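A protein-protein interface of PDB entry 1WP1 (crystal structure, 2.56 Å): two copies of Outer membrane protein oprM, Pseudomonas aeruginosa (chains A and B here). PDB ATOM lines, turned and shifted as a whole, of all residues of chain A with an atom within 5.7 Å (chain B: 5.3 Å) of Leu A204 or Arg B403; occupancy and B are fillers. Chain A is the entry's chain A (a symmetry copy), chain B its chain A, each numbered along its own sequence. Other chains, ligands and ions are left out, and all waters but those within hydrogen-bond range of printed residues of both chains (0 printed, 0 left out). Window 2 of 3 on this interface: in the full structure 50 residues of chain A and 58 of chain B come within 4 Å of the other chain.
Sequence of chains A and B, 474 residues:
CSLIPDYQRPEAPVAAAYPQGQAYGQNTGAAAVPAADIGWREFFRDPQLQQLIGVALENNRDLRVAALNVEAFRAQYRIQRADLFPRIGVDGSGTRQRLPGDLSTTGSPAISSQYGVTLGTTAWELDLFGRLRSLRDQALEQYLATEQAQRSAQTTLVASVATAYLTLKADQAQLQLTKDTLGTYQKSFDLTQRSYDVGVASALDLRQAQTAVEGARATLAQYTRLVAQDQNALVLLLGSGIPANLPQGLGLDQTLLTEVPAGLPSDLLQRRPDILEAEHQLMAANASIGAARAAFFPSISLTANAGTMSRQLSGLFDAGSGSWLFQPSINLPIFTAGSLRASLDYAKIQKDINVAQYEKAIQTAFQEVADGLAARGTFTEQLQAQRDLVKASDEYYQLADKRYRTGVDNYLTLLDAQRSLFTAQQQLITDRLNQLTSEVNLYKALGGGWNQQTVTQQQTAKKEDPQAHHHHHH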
ATOM      1  N   SER A 202      30.443  23.680 -32.533  1.00  0.00           N
ATOM      2  CA  SER A 202      29.323  22.773 -32.370  1.00  0.00           C
ATOM      3  C   SER A 202      28.408  23.184 -31.204  1.00  0.00           C
ATOM      4  O   SER A 202      28.813  23.937 -30.306  1.00  0.00           O
ATOM      5  CB  SER A 202      29.855  21.378 -32.120  1.00  0.00           C
ATOM      6  OG  SER A 202      30.528  21.330 -30.861  1.00  0.00           O
ATOM      7  N   ALA A 203      27.177  22.671 -31.233  1.00  0.00           N
ATOM      8  CA  ALA A 203      26.200  22.845 -30.162  1.00  0.00           C
ATOM      9  C   ALA A 203      26.800  22.417 -28.823  1.00  0.00           C
ATOM     10  O   ALA A 203      26.654  23.092 -27.811  1.00  0.00           O
ATOM     11  CB  ALA A 203      24.963  22.050 -30.474  1.00  0.00           C
ATOM     12  N   LEU A 204      27.507  21.296 -28.829  1.00  0.00           N
ATOM     13  CA  LEU A 204      28.211  20.816 -27.648  1.00  0.00           C
ATOM     14  C   LEU A 204      29.200  21.895 -27.126  1.00  0.00           C
ATOM     15  O   LEU A 204      29.164  22.246 -25.937  1.00  0.00           O
ATOM     16  CB  LEU A 204      28.879  19.459 -27.936  1.00  0.00           C
ATOM     17  CG  LEU A 204      29.618  18.861 -26.739  1.00  0.00           C
ATOM     18  CD1 LEU A 204      28.910  17.678 -26.099  1.00  0.00           C
ATOM     19  CD2 LEU A 204      31.019  18.486 -27.160  1.00  0.00           C
ATOM     20  N   ASP A 205      30.051  22.433 -27.997  1.00  0.00           N
ATOM     21  CA  ASP A 205      30.954  23.539 -27.609  1.00  0.00           C
ATOM     22  C   ASP A 205      30.202  24.640 -26.867  1.00  0.00           C
ATOM     23  O   ASP A 205      30.607  25.070 -25.794  1.00  0.00           O
ATOM     24  CB  ASP A 205      31.627  24.192 -28.824  1.00  0.00           C
ATOM     25  CG  ASP A 205      32.538  23.255 -29.581  1.00  0.00           C
ATOM     26  OD1 ASP A 205      33.020  22.273 -28.977  1.00  0.00           O
ATOM     27  OD2 ASP A 205      32.791  23.521 -30.785  1.00  0.00           O
ATOM     28  N   LEU A 206      29.100  25.075 -27.467  1.00  0.00           N
ATOM     29  CA  LEU A 206      28.248  26.120 -26.925  1.00  0.00           C
ATOM     30  C   LEU A 206      27.674  25.765 -25.542  1.00  0.00           C
ATOM     31  O   LEU A 206      27.705  26.588 -24.611  1.00  0.00           O
ATOM     32  CB  LEU A 206      27.141  26.451 -27.932  1.00  0.00           C
ATOM     33  CG  LEU A 206      26.445  27.802 -27.770  1.00  0.00           C
ATOM     34  CD1 LEU A 206      27.464  28.951 -27.852  1.00  0.00           C
ATOM     35  CD2 LEU A 206      25.293  27.997 -28.798  1.00  0.00           C
ATOM     36  N   ARG A 207      27.172  24.547 -25.380  1.00  0.00           N
ATOM     37  CA  ARG A 207      26.683  24.141 -24.070  1.00  0.00           C
ATOM     38  C   ARG A 207      27.825  24.144 -23.055  1.00  0.00           C
ATOM     39  O   ARG A 207      27.672  24.645 -21.929  1.00  0.00           O
ATOM     40  CB  ARG A 207      25.974  22.784 -24.132  1.00  0.00           C
ATOM     41  CG  ARG A 207      24.643  22.830 -24.892  1.00  0.00           C
ATOM     42  CD  ARG A 207      23.689  23.804 -24.198  1.00  0.00           C
ATOM     43  NE  ARG A 207      22.441  24.050 -24.938  1.00  0.00           N
ATOM     44  CZ  ARG A 207      21.378  24.684 -24.419  1.00  0.00           C
ATOM     45  NH1 ARG A 207      21.411  25.132 -23.152  1.00  0.00           N
ATOM     46  NH2 ARG A 207      20.279  24.873 -25.150  1.00  0.00           N
ATOM     47  N   GLN A 208      28.974  23.614 -23.446  1.00  0.00           N
ATOM     48  CA  GLN A 208      30.099  23.603 -22.533  1.00  0.00           C
ATOM     49  C   GLN A 208      30.428  25.003 -22.077  1.00  0.00           C
ATOM     50  O   GLN A 208      30.520  25.237 -20.876  1.00  0.00           O
ATOM     51  CB  GLN A 208      31.324  22.912 -23.122  1.00  0.00           C
ATOM     52  CG  GLN A 208      31.167  21.393 -23.164  1.00  0.00           C
ATOM     53  CD  GLN A 208      32.209  20.750 -24.024  1.00  0.00           C
ATOM     54  OE1 GLN A 208      32.377  21.135 -25.171  1.00  0.00           O
ATOM     55  NE2 GLN A 208      32.914  19.755 -23.486  1.00  0.00           N
ATOM     56  N   ALA A 209      30.575  25.926 -23.011  1.00  0.00           N
ATOM     57  CA  ALA A 209      30.856  27.316 -22.679  1.00  0.00           C
ATOM     58  C   ALA A 209      29.837  27.904 -21.688  1.00  0.00           C
ATOM     59  O   ALA A 209      30.212  28.551 -20.709  1.00  0.00           O
ATOM     60  CB  ALA A 209      30.906  28.146 -23.946  1.00  0.00           C
ATOM     61  N   TYR B 396      24.097  19.606 -21.918  1.00  0.00           N
ATOM     62  CA  TYR B 396      25.457  19.144 -22.177  1.00  0.00           C
ATOM     63  C   TYR B 396      25.457  17.615 -22.159  1.00  0.00           C
ATOM     64  O   TYR B 396      25.959  16.946 -23.076  1.00  0.00           O
ATOM     65  CB  TYR B 396      26.359  19.713 -21.092  1.00  0.00           C
ATOM     66  CG  TYR B 396      27.818  19.308 -21.082  1.00  0.00           C
ATOM     67  CD1 TYR B 396      28.450  18.825 -22.222  1.00  0.00           C
ATOM     68  CD2 TYR B 396      28.589  19.486 -19.917  1.00  0.00           C
ATOM     69  CE1 TYR B 396      29.811  18.463 -22.204  1.00  0.00           C
ATOM     70  CE2 TYR B 396      29.964  19.140 -19.884  1.00  0.00           C
ATOM     71  CZ  TYR B 396      30.555  18.639 -21.047  1.00  0.00           C
ATOM     72  OH  TYR B 396      31.863  18.299 -21.048  1.00  0.00           O
ATOM     73  N   GLN B 398      22.874  15.501 -22.546  1.00  0.00           N
ATOM     74  CA  GLN B 398      22.095  14.868 -23.612  1.00  0.00           C
ATOM     75  C   GLN B 398      22.907  14.743 -24.884  1.00  0.00           C
ATOM     76  O   GLN B 398      23.009  13.646 -25.449  1.00  0.00           O
ATOM     77  CB  GLN B 398      20.749  15.567 -23.857  1.00  0.00           C
ATOM     78  CG  GLN B 398      19.685  15.191 -22.824  1.00  0.00           C
ATOM     79  CD  GLN B 398      18.580  16.248 -22.703  1.00  0.00           C
ATOM     80  OE1 GLN B 398      18.026  16.726 -23.706  1.00  0.00           O
ATOM     81  NE2 GLN B 398      18.251  16.617 -21.456  1.00  0.00           N
ATOM     82  N   LEU B 399      23.510  15.852 -25.301  1.00  0.00           N
ATOM     83  CA  LEU B 399      24.440  15.856 -26.424  1.00  0.00           C
ATOM     84  C   LEU B 399      25.604  14.862 -26.287  1.00  0.00           C
ATOM     85  O   LEU B 399      25.801  14.008 -27.156  1.00  0.00           O
ATOM     86  CB  LEU B 399      24.962  17.272 -26.679  1.00  0.00           C
ATOM     87  CG  LEU B 399      24.033  18.036 -27.632  1.00  0.00           C
ATOM     88  CD1 LEU B 399      24.325  19.529 -27.602  1.00  0.00           C
ATOM     89  CD2 LEU B 399      24.074  17.472 -29.084  1.00  0.00           C
ATOM     90  N   ALA B 400      26.355  14.954 -25.197  1.00  0.00           N
ATOM     91  CA  ALA B 400      27.500  14.078 -24.992  1.00  0.00           C
ATOM     92  C   ALA B 400      27.131  12.599 -25.079  1.00  0.00           C
ATOM     93  O   ALA B 400      27.853  11.834 -25.702  1.00  0.00           O
ATOM     94  CB  ALA B 400      28.179  14.385 -23.680  1.00  0.00           C
ATOM     95  N   ASP B 401      26.008  12.196 -24.478  1.00  0.00           N
ATOM     96  CA  ASP B 401      25.591  10.794 -24.563  1.00  0.00           C
ATOM     97  C   ASP B 401      25.299  10.432 -26.015  1.00  0.00           C
ATOM     98  O   ASP B 401      25.809   9.436 -26.519  1.00  0.00           O
ATOM     99  CB  ASP B 401      24.396  10.480 -23.654  1.00  0.00           C
ATOM    100  CG  ASP B 401      24.169   8.972 -23.476  1.00  0.00           C
ATOM    101  OD1 ASP B 401      23.476   8.361 -24.317  1.00  0.00           O
ATOM    102  OD2 ASP B 401      24.683   8.387 -22.495  1.00  0.00           O
ATOM    103  N   LYS B 402      24.515  11.256 -26.695  1.00  0.00           N
ATOM    104  CA  LYS B 402      24.252  11.037 -28.107  1.00  0.00           C
ATOM    105  C   LYS B 402      25.544  10.927 -28.935  1.00  0.00           C
ATOM    106  O   LYS B 402      25.735   9.938 -29.657  1.00  0.00           O
ATOM    107  CB  LYS B 402      23.302  12.112 -28.670  1.00  0.00           C
ATOM    108  CG  LYS B 402      23.228  12.156 -30.206  1.00  0.00           C
ATOM    109  CD  LYS B 402      22.419  13.346 -30.684  1.00  0.00           C
ATOM    110  CE  LYS B 402      22.479  13.473 -32.205  1.00  0.00           C
ATOM    111  NZ  LYS B 402      21.181  14.019 -32.717  1.00  0.00           N
ATOM    112  N   ARG B 403      26.423  11.926 -28.834  1.00  0.00           N
ATOM    113  CA  ARG B 403      27.698  11.924 -29.582  1.00  0.00           C
ATOM    114  C   ARG B 403      28.563  10.690 -29.270  1.00  0.00           C
ATOM    115  O   ARG B 403      29.252  10.182 -30.156  1.00  0.00           O
ATOM    116  CB  ARG B 403      28.507  13.213 -29.357  1.00  0.00           C
ATOM    117  CG  ARG B 403      27.751  14.513 -29.674  1.00  0.00           C
ATOM    118  CD  ARG B 403      28.642  15.762 -29.675  1.00  0.00           C
ATOM    119  NE  ARG B 403      29.430  15.855 -30.906  1.00  0.00           N
ATOM    120  CZ  ARG B 403      30.758  15.935 -30.937  1.00  0.00           C
ATOM    121  NH1 ARG B 403      31.449  15.972 -29.812  1.00  0.00           N
ATOM    122  NH2 ARG B 403      31.405  15.978 -32.095  1.00  0.00           N
ATOM    123  N   TYR B 404      28.509  10.205 -28.026  1.00  0.00           N
ATOM    124  CA  TYR B 404      29.211   8.976 -27.670  1.00  0.00           C
ATOM    125  C   TYR B 404      28.624   7.712 -28.342  1.00  0.00           C
ATOM    126  O   TYR B 404      29.368   6.939 -28.950  1.00  0.00           O
ATOM    127  CB  TYR B 404      29.406   8.744 -26.148  1.00  0.00           C
ATOM    128  CG  TYR B 404      30.050   7.368 -25.966  1.00  0.00           C
ATOM    129  CD1 TYR B 404      31.396   7.156 -26.351  1.00  0.00           C
ATOM    130  CD2 TYR B 404      29.293   6.256 -25.546  1.00  0.00           C
ATOM    131  CE1 TYR B 404      31.983   5.910 -26.298  1.00  0.00           C
ATOM    132  CE2 TYR B 404      29.874   5.010 -25.471  1.00  0.00           C
ATOM    133  CZ  TYR B 404      31.236   4.841 -25.851  1.00  0.00           C
ATOM    134  OH  TYR B 404      31.837   3.601 -25.780  1.00  0.00           O
ATOM    135  N   ARG B 405      27.314   7.498 -28.178  1.00  0.00           N
ATOM    136  CA  ARG B 405      26.601   6.316 -28.730  1.00  0.00           C
ATOM    137  C   ARG B 405      26.761   6.194 -30.244  1.00  0.00           C
ATOM    138  O   ARG B 405      26.784   5.113 -30.803  1.00  0.00           O
ATOM    139  CB  ARG B 405      25.096   6.381 -28.398  1.00  0.00           C
ATOM    140  CG  ARG B 405      24.764   6.433 -26.908  1.00  0.00           C
ATOM    141  CD  ARG B 405      25.316   5.230 -26.185  1.00  0.00           C
ATOM    142  NE  ARG B 405      25.422   5.475 -24.748  1.00  0.00           N
ATOM    143  CZ  ARG B 405      26.164   4.747 -23.913  1.00  0.00           C
ATOM    144  NH1 ARG B 405      26.886   3.723 -24.369  1.00  0.00           N
ATOM    145  NH2 ARG B 405      26.175   5.039 -22.628  1.00  0.00           N
ATOM    146  N   THR B 406      26.893   7.334 -30.889  1.00  0.00           N
ATOM    147  CA  THR B 406      26.825   7.437 -32.317  1.00  0.00           C
ATOM    148  C   THR B 406      28.225   7.297 -32.900  1.00  0.00           C
ATOM    149  O   THR B 406      28.408   7.302 -34.109  1.00  0.00           O
ATOM    150  CB  THR B 406      26.146   8.808 -32.646  1.00  0.00           C
ATOM    151  OG1 THR B 406      24.733   8.613 -32.754  1.00  0.00           O
ATOM    152  CG2 THR B 406      26.663   9.443 -33.913  1.00  0.00           C
ATOM    153  N   GLY B 407      29.221   7.168 -32.039  1.00  0.00           N
ATOM    154  CA  GLY B 407      30.592   7.029 -32.494  1.00  0.00           C
ATOM    155  C   GLY B 407      31.201   8.366 -32.854  1.00  0.00           C
ATOM    156  O   GLY B 407      32.411   8.455 -33.113  1.00  0.00           O
ATOM    157  N   VAL B 408      30.388   9.427 -32.843  1.00  0.00           N
ATOM    158  CA  VAL B 408      30.904  10.741 -33.198  1.00  0.00           C
ATOM    159  C   VAL B 408      31.965  11.290 -32.224  1.00  0.00           C
ATOM    160  O   VAL B 408      32.824  12.085 -32.642  1.00  0.00           O
ATOM    161  CB  VAL B 408      29.752  11.742 -33.504  1.00  0.00           C
ATOM    162  CG1 VAL B 408      30.133  13.202 -33.191  1.00  0.00           C
ATOM    163  CG2 VAL B 408      29.294  11.585 -34.965  1.00  0.00           C
ATOM    164  N   ASP B 409      31.934  10.854 -30.954  1.00  0.00           N
ATOM    165  CA  ASP B 409      32.805  11.422 -29.884  1.00  0.00           C
ATOM    166  C   ASP B 409      33.105  10.468 -28.696  1.00  0.00           C
ATOM    167  O   ASP B 409      32.460   9.410 -28.568  1.00  0.00           O
ATOM    168  CB  ASP B 409      32.188  12.736 -29.392  1.00  0.00           C
ATOM    169  CG  ASP B 409      33.219  13.700 -28.826  1.00  0.00           C
ATOM    170  OD1 ASP B 409      34.378  13.288 -28.669  1.00  0.00           O
ATOM    171  OD2 ASP B 409      32.873  14.877 -28.524  1.00  0.00           O
ATOM    172  N   THR B 413      34.084  12.914 -22.541  1.00  0.00           N
ATOM    173  CA  THR B 413      33.146  14.019 -22.596  1.00  0.00           C
ATOM    174  C   THR B 413      31.871  13.608 -21.910  1.00  0.00           C
ATOM    175  O   THR B 413      31.313  14.383 -21.105  1.00  0.00           O
ATOM    176  CB  THR B 413      32.834  14.486 -24.045  1.00  0.00           C
ATOM    177  OG1 THR B 413      34.056  14.760 -24.730  1.00  0.00           O
ATOM    178  CG2 THR B 413      31.995  15.761 -24.045  1.00  0.00           C
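The side-chain hydroxyl of Tyr B396 lies within hydrogen-bond range of the side-chain amide nitrogen of Gln A208 (3.0 Å).
Of the printed residues of chain B, Ala A203 touches Leu B399. Printed residues of chain B within 4 Å of Leu A204: Leu B399 (3.8 Å), Ala B400 (3.8 Å) and Arg B403 (3.7 Å). Arg A207 touches none of the printed residues of chain B. Printed residues of chain B within 4 Å of Gln A208: Tyr B396. Printed residues of chain A within 4 Å of Tyr B396: Gln A208 (3.0 Å). Of the printed residues of chain A, Ala B400 touches Leu A204. The nearest residue of chain A that does not touch Arg B403 is Ser A202 (5.4 Å). The nearest printed residue of chain B that does not touch Gln A208 is Thr B413 (4.1 Å).
The backbone carbonyl oxygen (O) of Leu A204 lies close to the side-chain amide oxygen (OE1) of Gln A208, 3.5 Å away. O of Arg B403 is in hydrogen-bond range of N of Val B408 (3.0 Å). O of Arg B403 lies within hydrogen-bond range of N of Asp B409 (2.9 Å).
No position is printed for both chains. Of the 5 pairs that touch across the chains among the printed residues, none has its exchanged pair printed and touching as well.
Among the printed residues, pairs that only touch across the chains: Ala A203 with Leu B399 (3.9 Å), Leu A204 with Leu B399 (3.8 Å), Leu A204 with Ala B400 (3.8 Å) and Leu A204 with Arg B403 (3.7 Å).
Printed residues of chain A that touch a printed residue of chain B: Ala A203, Leu A204 and Gln A208. Hydrophobic or aromatic side chains of chain A that line the printed part of chain B: Ala A203 and Leu A204. Hydrophobic or aromatic side chains of chain B that line the printed part of chain A: Tyr B396 and Leu B399. Among the printed residues, 5 pairs touch across the chains.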
